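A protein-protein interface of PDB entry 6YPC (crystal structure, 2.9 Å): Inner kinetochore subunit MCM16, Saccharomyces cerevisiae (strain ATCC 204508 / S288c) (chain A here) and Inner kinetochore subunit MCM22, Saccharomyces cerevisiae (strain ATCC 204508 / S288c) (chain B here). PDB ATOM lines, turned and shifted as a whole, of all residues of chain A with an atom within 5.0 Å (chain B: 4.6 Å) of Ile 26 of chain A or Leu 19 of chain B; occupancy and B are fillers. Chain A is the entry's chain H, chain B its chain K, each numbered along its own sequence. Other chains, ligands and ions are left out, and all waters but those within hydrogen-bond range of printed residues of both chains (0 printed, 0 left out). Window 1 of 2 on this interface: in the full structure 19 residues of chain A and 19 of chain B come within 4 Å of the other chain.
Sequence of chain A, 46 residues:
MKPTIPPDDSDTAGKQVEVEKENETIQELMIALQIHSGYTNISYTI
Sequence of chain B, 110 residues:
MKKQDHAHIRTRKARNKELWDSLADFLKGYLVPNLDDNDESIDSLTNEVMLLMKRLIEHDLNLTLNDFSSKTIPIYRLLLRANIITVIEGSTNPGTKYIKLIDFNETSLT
Among the printed residues, pairs that only touch across the chains: Ile 46 of chain A with Leu 19 of chain B, Asn 23 of chain A with Leu 19 of chain B, Thr 25 of chain A with Ile 57 of chain B, Ile 26 of chain A with Trp 20 of chain B, Leu 29 of chain A with Ile 57 of chain B, Ile 46 of chain A with Arg 15 of chain B, Ile 26 of chain A with Leu 19 of chain B, Ile 26 of chain A with Ile 57 of chain B, Asn 23 of chain A with Arg 15 of chain B and Gln 27 of chain A with Arg 15 of chain B.
Of the 10 printed residues of chain B, 7 touch a printed residue of chain A.
Hydrophobic or aromatic side chains of chain B within 4 Å of the printed part of chain A: Leu 19, Trp 20, Leu 23 and Ile 57.
Hydrophobic or aromatic side chains of chain A within 4 Å of the printed part of chain B: Ile 26, Leu 29 and Met 30.
Along chain A the printed residues that touch a printed residue of chain B span positions 22 to 46.
Among the printed residues, no Asp or Glu carboxylate lies within 4 Å of a Lys or Arg side-chain nitrogen of the other chain.
Ile 26 of chain A touches just these residues of chain B: Leu 19, Trp 20 and Ile 57.
Leu 19 of chain B touches just these residues of chain A: Asn 23 (3.4 Å), Ile 26 (3.7 Å) and Ile 46 (3.2 Å).
Of the printed residues of chain A, Leu 23 of chain B touches Met 30.
Of the printed residues of chain A, Trp 20 of chain B touches Glu 22 and Ile 26.
The nearest printed residue of chain B that does not touch Leu 29 of chain A is Leu 23 of chain B (4.5 Å).
NE1 of Trp 20 of chain B sits close to OD1 of Asn 16 of chain B (3.3 Å).
The backbone carbonyl oxygen (O) of Glu 22 of chain A lies within hydrogen-bond range of the side-chain hydroxyl (OG1) of Thr 25 of chain A, 3.4 Å away.
The side-chain amide nitrogen of Asn 16 of chain B is in hydrogen-bond range of the side-chain carboxylate of Glu 22 of chain A, 2.6 Å away.
The side-chain amide oxygen of Asn 23 of chain A is in hydrogen-bond range of the side-chain amide nitrogen of Asn 16 of chain B, 3.0 Å away.
The side-chain carboxylate of Glu 22 of chain A lies within hydrogen-bond range of the indole nitrogen of Trp 20 of chain B (2.9 Å).
OG of Ser 22 of chain B is in hydrogen-bond range of SD of Met 30 of chain A (3.3 Å).
N of Leu 23 of chain B lies close to SD of Met 30 of chain A (3.6 Å).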
ATOM      1  N   GLU A  22      30.312   0.240  -1.048  1.00  0.00           N
ATOM      2  CA  GLU A  22      28.978  -0.042  -0.542  1.00  0.00           C
ATOM      3  C   GLU A  22      28.883  -1.482  -0.097  1.00  0.00           C
ATOM      4  O   GLU A  22      28.115  -1.792   0.819  1.00  0.00           O
ATOM      5  CB  GLU A  22      27.905   0.268  -1.582  1.00  0.00           C
ATOM      6  CG  GLU A  22      27.443  -0.925  -2.384  1.00  0.00           C
ATOM      7  CD  GLU A  22      26.143  -0.674  -3.141  1.00  0.00           C
ATOM      8  OE1 GLU A  22      25.606   0.452  -3.035  1.00  0.00           O
ATOM      9  OE2 GLU A  22      25.675  -1.600  -3.859  1.00  0.00           O
ATOM     10  N   ASN A  23      29.660  -2.368  -0.726  1.00  0.00           N
ATOM     11  CA  ASN A  23      29.882  -3.687  -0.150  1.00  0.00           C
ATOM     12  C   ASN A  23      30.293  -3.556   1.309  1.00  0.00           C
ATOM     13  O   ASN A  23      29.805  -4.293   2.165  1.00  0.00           O
ATOM     14  CB  ASN A  23      30.954  -4.450  -0.943  1.00  0.00           C
ATOM     15  CG  ASN A  23      30.367  -5.358  -2.007  1.00  0.00           C
ATOM     16  OD1 ASN A  23      29.176  -5.297  -2.305  1.00  0.00           O
ATOM     17  ND2 ASN A  23      31.216  -6.196  -2.600  1.00  0.00           N
ATOM     18  N   GLU A  24      31.164  -2.593   1.619  1.00  0.00           N
ATOM     19  CA  GLU A  24      31.643  -2.477   2.990  1.00  0.00           C
ATOM     20  C   GLU A  24      30.573  -1.913   3.916  1.00  0.00           C
ATOM     21  O   GLU A  24      30.476  -2.328   5.079  1.00  0.00           O
ATOM     22  CB  GLU A  24      32.913  -1.625   3.062  1.00  0.00           C
ATOM     23  CG  GLU A  24      33.501  -1.556   4.482  1.00  0.00           C
ATOM     24  CD  GLU A  24      33.619  -2.952   5.161  1.00  0.00           C
ATOM     25  OE1 GLU A  24      33.960  -3.961   4.473  1.00  0.00           O
ATOM     26  OE2 GLU A  24      33.368  -3.039   6.393  1.00  0.00           O
ATOM     27  N   THR A  25      29.754  -0.976   3.443  1.00  0.00           N
ATOM     28  CA  THR A  25      28.827  -0.403   4.407  1.00  0.00           C
ATOM     29  C   THR A  25      27.663  -1.348   4.704  1.00  0.00           C
ATOM     30  O   THR A  25      27.297  -1.508   5.873  1.00  0.00           O
ATOM     31  CB  THR A  25      28.340   0.962   3.937  1.00  0.00           C
ATOM     32  OG1 THR A  25      27.408   0.788   2.871  1.00  0.00           O
ATOM     33  CG2 THR A  25      29.499   1.794   3.456  1.00  0.00           C
ATOM     34  N   ILE A  26      27.077  -1.997   3.688  1.00  0.00           N
ATOM     35  CA  ILE A  26      26.030  -2.990   3.955  1.00  0.00           C
ATOM     36  C   ILE A  26      26.502  -3.985   5.003  1.00  0.00           C
ATOM     37  O   ILE A  26      25.786  -4.299   5.963  1.00  0.00           O
ATOM     38  CB  ILE A  26      25.619  -3.729   2.672  1.00  0.00           C
ATOM     39  CG1 ILE A  26      25.086  -2.757   1.612  1.00  0.00           C
ATOM     40  CG2 ILE A  26      24.593  -4.812   3.023  1.00  0.00           C
ATOM     41  CD1 ILE A  26      24.693  -3.450   0.269  1.00  0.00           C
ATOM     42  N   GLN A  27      27.718  -4.504   4.830  1.00  0.00           N
ATOM     43  CA  GLN A  27      28.270  -5.426   5.812  1.00  0.00           C
ATOM     44  C   GLN A  27      28.261  -4.800   7.201  1.00  0.00           C
ATOM     45  O   GLN A  27      27.646  -5.327   8.135  1.00  0.00           O
ATOM     46  CB  GLN A  27      29.688  -5.848   5.413  1.00  0.00           C
ATOM     47  CG  GLN A  27      30.241  -7.016   6.236  1.00  0.00           C
ATOM     48  CD  GLN A  27      31.564  -7.579   5.700  1.00  0.00           C
ATOM     49  OE1 GLN A  27      31.583  -8.349   4.732  1.00  0.00           O
ATOM     50  NE2 GLN A  27      32.673  -7.200   6.340  1.00  0.00           N
ATOM     51  N   GLU A  28      28.911  -3.650   7.352  1.00  0.00           N
ATOM     52  CA  GLU A  28      28.960  -3.053   8.676  1.00  0.00           C
ATOM     53  C   GLU A  28      27.586  -2.622   9.164  1.00  0.00           C
ATOM     54  O   GLU A  28      27.371  -2.564  10.377  1.00  0.00           O
ATOM     55  CB  GLU A  28      29.928  -1.878   8.677  1.00  0.00           C
ATOM     56  CG  GLU A  28      31.402  -2.310   8.659  1.00  0.00           C
ATOM     57  CD  GLU A  28      31.759  -3.243   9.819  1.00  0.00           C
ATOM     58  OE1 GLU A  28      32.604  -4.167   9.628  1.00  0.00           O
ATOM     59  OE2 GLU A  28      31.171  -3.055  10.915  1.00  0.00           O
ATOM     60  N   LEU A  29      26.653  -2.347   8.251  1.00  0.00           N
ATOM     61  CA  LEU A  29      25.302  -1.963   8.649  1.00  0.00           C
ATOM     62  C   LEU A  29      24.562  -3.146   9.256  1.00  0.00           C
ATOM     63  O   LEU A  29      23.925  -3.019  10.312  1.00  0.00           O
ATOM     64  CB  LEU A  29      24.536  -1.404   7.448  1.00  0.00           C
ATOM     65  CG  LEU A  29      23.082  -0.942   7.610  1.00  0.00           C
ATOM     66  CD1 LEU A  29      22.958   0.265   8.540  1.00  0.00           C
ATOM     67  CD2 LEU A  29      22.516  -0.577   6.257  1.00  0.00           C
ATOM     68  N   MET A  30      24.655  -4.317   8.617  1.00  0.00           N
ATOM     69  CA  MET A  30      23.921  -5.471   9.120  1.00  0.00           C
ATOM     70  C   MET A  30      24.402  -5.854  10.515  1.00  0.00           C
ATOM     71  O   MET A  30      23.597  -5.962  11.449  1.00  0.00           O
ATOM     72  CB  MET A  30      24.028  -6.638   8.142  1.00  0.00           C
ATOM     73  CG  MET A  30      23.466  -6.311   6.764  1.00  0.00           C
ATOM     74  SD  MET A  30      22.809  -7.745   5.868  1.00  0.00           S
ATOM     75  CE  MET A  30      21.552  -8.340   6.999  1.00  0.00           C
ATOM     76  N   THR A  45      28.122 -14.166   6.772  1.00  0.00           N
ATOM     77  CA  THR A  45      27.501 -14.274   5.455  1.00  0.00           C
ATOM     78  C   THR A  45      28.473 -13.809   4.366  1.00  0.00           C
ATOM     79  O   THR A  45      29.255 -12.872   4.578  1.00  0.00           O
ATOM     80  CB  THR A  45      26.210 -13.446   5.387  1.00  0.00           C
ATOM     81  OG1 THR A  45      25.711 -13.439   4.041  1.00  0.00           O
ATOM     82  CG2 THR A  45      26.457 -11.993   5.841  1.00  0.00           C
ATOM     83  N   ILE A  46      28.426 -14.474   3.202  1.00  0.00           N
ATOM     84  CA  ILE A  46      29.275 -14.113   2.050  1.00  0.00           C
ATOM     85  C   ILE A  46      28.585 -13.026   1.204  1.00  0.00           C
ATOM     86  O   ILE A  46      28.713 -11.824   1.480  1.00  0.00           O
ATOM     87  CB  ILE A  46      29.637 -15.366   1.177  1.00  0.00           C
ATOM     88  CG1 ILE A  46      30.808 -15.058   0.231  1.00  0.00           C
ATOM     89  CG2 ILE A  46      28.423 -15.872   0.396  1.00  0.00           C
ATOM     90  CD1 ILE A  46      31.031 -16.115  -0.837  1.00  0.00           C
ATOM     91  N   ARG B  15      29.162 -10.519  -4.959  1.00  0.00           N
ATOM     92  CA  ARG B  15      28.997 -10.267  -3.531  1.00  0.00           C
ATOM     93  C   ARG B  15      28.036  -9.119  -3.265  1.00  0.00           C
ATOM     94  O   ARG B  15      27.315  -9.133  -2.260  1.00  0.00           O
ATOM     95  CB  ARG B  15      30.341  -9.962  -2.879  1.00  0.00           C
ATOM     96  CG  ARG B  15      30.303 -10.092  -1.380  1.00  0.00           C
ATOM     97  CD  ARG B  15      31.565  -9.548  -0.752  1.00  0.00           C
ATOM     98  NE  ARG B  15      31.708  -9.980   0.636  1.00  0.00           N
ATOM     99  CZ  ARG B  15      32.454 -11.016   1.017  1.00  0.00           C
ATOM    100  NH1 ARG B  15      33.127 -11.741   0.118  1.00  0.00           N
ATOM    101  NH2 ARG B  15      32.524 -11.334   2.299  1.00  0.00           N
ATOM    102  N   ASN B  16      28.003  -8.120  -4.149  1.00  0.00           N
ATOM    103  CA  ASN B  16      27.128  -6.986  -3.904  1.00  0.00           C
ATOM    104  C   ASN B  16      25.663  -7.383  -3.968  1.00  0.00           C
ATOM    105  O   ASN B  16      24.863  -6.887  -3.171  1.00  0.00           O
ATOM    106  CB  ASN B  16      27.393  -5.853  -4.885  1.00  0.00           C
ATOM    107  CG  ASN B  16      26.561  -4.624  -4.566  1.00  0.00           C
ATOM    108  OD1 ASN B  16      25.406  -4.513  -4.976  1.00  0.00           O
ATOM    109  ND2 ASN B  16      27.143  -3.698  -3.821  1.00  0.00           N
ATOM    110  N   LYS B  17      25.259  -8.243  -4.910  1.00  0.00           N
ATOM    111  CA  LYS B  17      23.854  -8.615  -4.796  1.00  0.00           C
ATOM    112  C   LYS B  17      23.647  -9.557  -3.622  1.00  0.00           C
ATOM    113  O   LYS B  17      22.602  -9.494  -2.958  1.00  0.00           O
ATOM    114  CB  LYS B  17      23.297  -9.227  -6.084  1.00  0.00           C
ATOM    115  CG  LYS B  17      21.746  -9.399  -6.048  1.00  0.00           C
ATOM    116  CD  LYS B  17      21.024  -8.324  -5.161  1.00  0.00           C
ATOM    117  CE  LYS B  17      19.821  -7.603  -5.805  1.00  0.00           C
ATOM    118  NZ  LYS B  17      18.993  -6.839  -4.794  1.00  0.00           N
ATOM    119  N   GLU B  18      24.639 -10.380  -3.292  1.00  0.00           N
ATOM    120  CA  GLU B  18      24.358 -11.286  -2.196  1.00  0.00           C
ATOM    121  C   GLU B  18      24.372 -10.585  -0.841  1.00  0.00           C
ATOM    122  O   GLU B  18      23.962 -11.206   0.148  1.00  0.00           O
ATOM    123  CB  GLU B  18      25.305 -12.486  -2.227  1.00  0.00           C
ATOM    124  CG  GLU B  18      24.585 -13.808  -1.830  1.00  0.00           C
ATOM    125  CD  GLU B  18      23.418 -14.229  -2.774  1.00  0.00           C
ATOM    126  OE1 GLU B  18      23.496 -14.014  -4.014  1.00  0.00           O
ATOM    127  OE2 GLU B  18      22.413 -14.780  -2.257  1.00  0.00           O
ATOM    128  N   LEU B  19      24.778  -9.310  -0.772  1.00  0.00           N
ATOM    129  CA  LEU B  19      24.534  -8.521   0.435  1.00  0.00           C
ATOM    130  C   LEU B  19      23.169  -7.841   0.391  1.00  0.00           C
ATOM    131  O   LEU B  19      22.444  -7.841   1.393  1.00  0.00           O
ATOM    132  CB  LEU B  19      25.640  -7.491   0.631  1.00  0.00           C
ATOM    133  CG  LEU B  19      26.996  -8.132   0.876  1.00  0.00           C
ATOM    134  CD1 LEU B  19      28.005  -7.131   1.387  1.00  0.00           C
ATOM    135  CD2 LEU B  19      26.821  -9.240   1.863  1.00  0.00           C
ATOM    136  N   TRP B  20      22.802  -7.265  -0.765  1.00  0.00           N
ATOM    137  CA  TRP B  20      21.513  -6.585  -0.893  1.00  0.00           C
ATOM    138  C   TRP B  20      20.361  -7.504  -0.539  1.00  0.00           C
ATOM    139  O   TRP B  20      19.471  -7.127   0.234  1.00  0.00           O
ATOM    140  CB  TRP B  20      21.335  -6.016  -2.305  1.00  0.00           C
ATOM    141  CG  TRP B  20      21.948  -4.646  -2.415  1.00  0.00           C
ATOM    142  CD1 TRP B  20      23.082  -4.300  -3.095  1.00  0.00           C
ATOM    143  CD2 TRP B  20      21.489  -3.451  -1.772  1.00  0.00           C
ATOM    144  NE1 TRP B  20      23.341  -2.963  -2.928  1.00  0.00           N
ATOM    145  CE2 TRP B  20      22.380  -2.421  -2.114  1.00  0.00           C
ATOM    146  CE3 TRP B  20      20.415  -3.156  -0.938  1.00  0.00           C
ATOM    147  CZ2 TRP B  20      22.226  -1.112  -1.648  1.00  0.00           C
ATOM    148  CZ3 TRP B  20      20.263  -1.856  -0.484  1.00  0.00           C
ATOM    149  CH2 TRP B  20      21.163  -0.853  -0.841  1.00  0.00           C
ATOM    150  N   ASP B  21      20.374  -8.728  -1.064  1.00  0.00           N
ATOM    151  CA  ASP B  21      19.260  -9.620  -0.781  1.00  0.00           C
ATOM    152  C   ASP B  21      19.410 -10.249   0.600  1.00  0.00           C
ATOM    153  O   ASP B  21      18.421 -10.635   1.228  1.00  0.00           O
ATOM    154  CB  ASP B  21      19.143 -10.675  -1.874  1.00  0.00           C
ATOM    155  CG  ASP B  21      20.408 -11.478  -2.038  1.00  0.00           C
ATOM    156  OD1 ASP B  21      20.437 -12.295  -2.996  1.00  0.00           O
ATOM    157  OD2 ASP B  21      21.337 -11.340  -1.200  1.00  0.00           O
ATOM    158  N   SER B  22      20.635 -10.330   1.109  1.00  0.00           N
ATOM    159  CA  SER B  22      20.807 -10.735   2.497  1.00  0.00           C
ATOM    160  C   SER B  22      20.213  -9.696   3.429  1.00  0.00           C
ATOM    161  O   SER B  22      19.470 -10.026   4.355  1.00  0.00           O
ATOM    162  CB  SER B  22      22.282 -10.931   2.817  1.00  0.00           C
ATOM    163  OG  SER B  22      22.518 -10.587   4.160  1.00  0.00           O
ATOM    164  N   LEU B  23      20.520  -8.428   3.193  1.00  0.00           N
ATOM    165  CA  LEU B  23      19.882  -7.373   3.961  1.00  0.00           C
ATOM    166  C   LEU B  23      18.381  -7.429   3.786  1.00  0.00           C
ATOM    167  O   LEU B  23      17.624  -7.342   4.757  1.00  0.00           O
ATOM    168  CB  LEU B  23      20.416  -6.022   3.514  1.00  0.00           C
ATOM    169  CG  LEU B  23      19.735  -4.870   4.219  1.00  0.00           C
ATOM    170  CD1 LEU B  23      20.479  -4.543   5.466  1.00  0.00           C
ATOM    171  CD2 LEU B  23      19.703  -3.709   3.283  1.00  0.00           C
ATOM    172  N   ILE B  57      22.230   3.683   2.821  1.00  0.00           N
ATOM    173  CA  ILE B  57      23.450   3.081   2.291  1.00  0.00           C
ATOM    174  C   ILE B  57      24.025   3.931   1.171  1.00  0.00           C
ATOM    175  O   ILE B  57      25.241   4.112   1.070  1.00  0.00           O
ATOM    176  CB  ILE B  57      23.175   1.644   1.819  1.00  0.00           C
ATOM    177  CG1 ILE B  57      22.755   0.769   2.988  1.00  0.00           C
ATOM    178  CG2 ILE B  57      24.400   1.052   1.182  1.00  0.00           C
ATOM    179  CD1 ILE B  57      22.158  -0.566   2.570  1.00  0.00           C
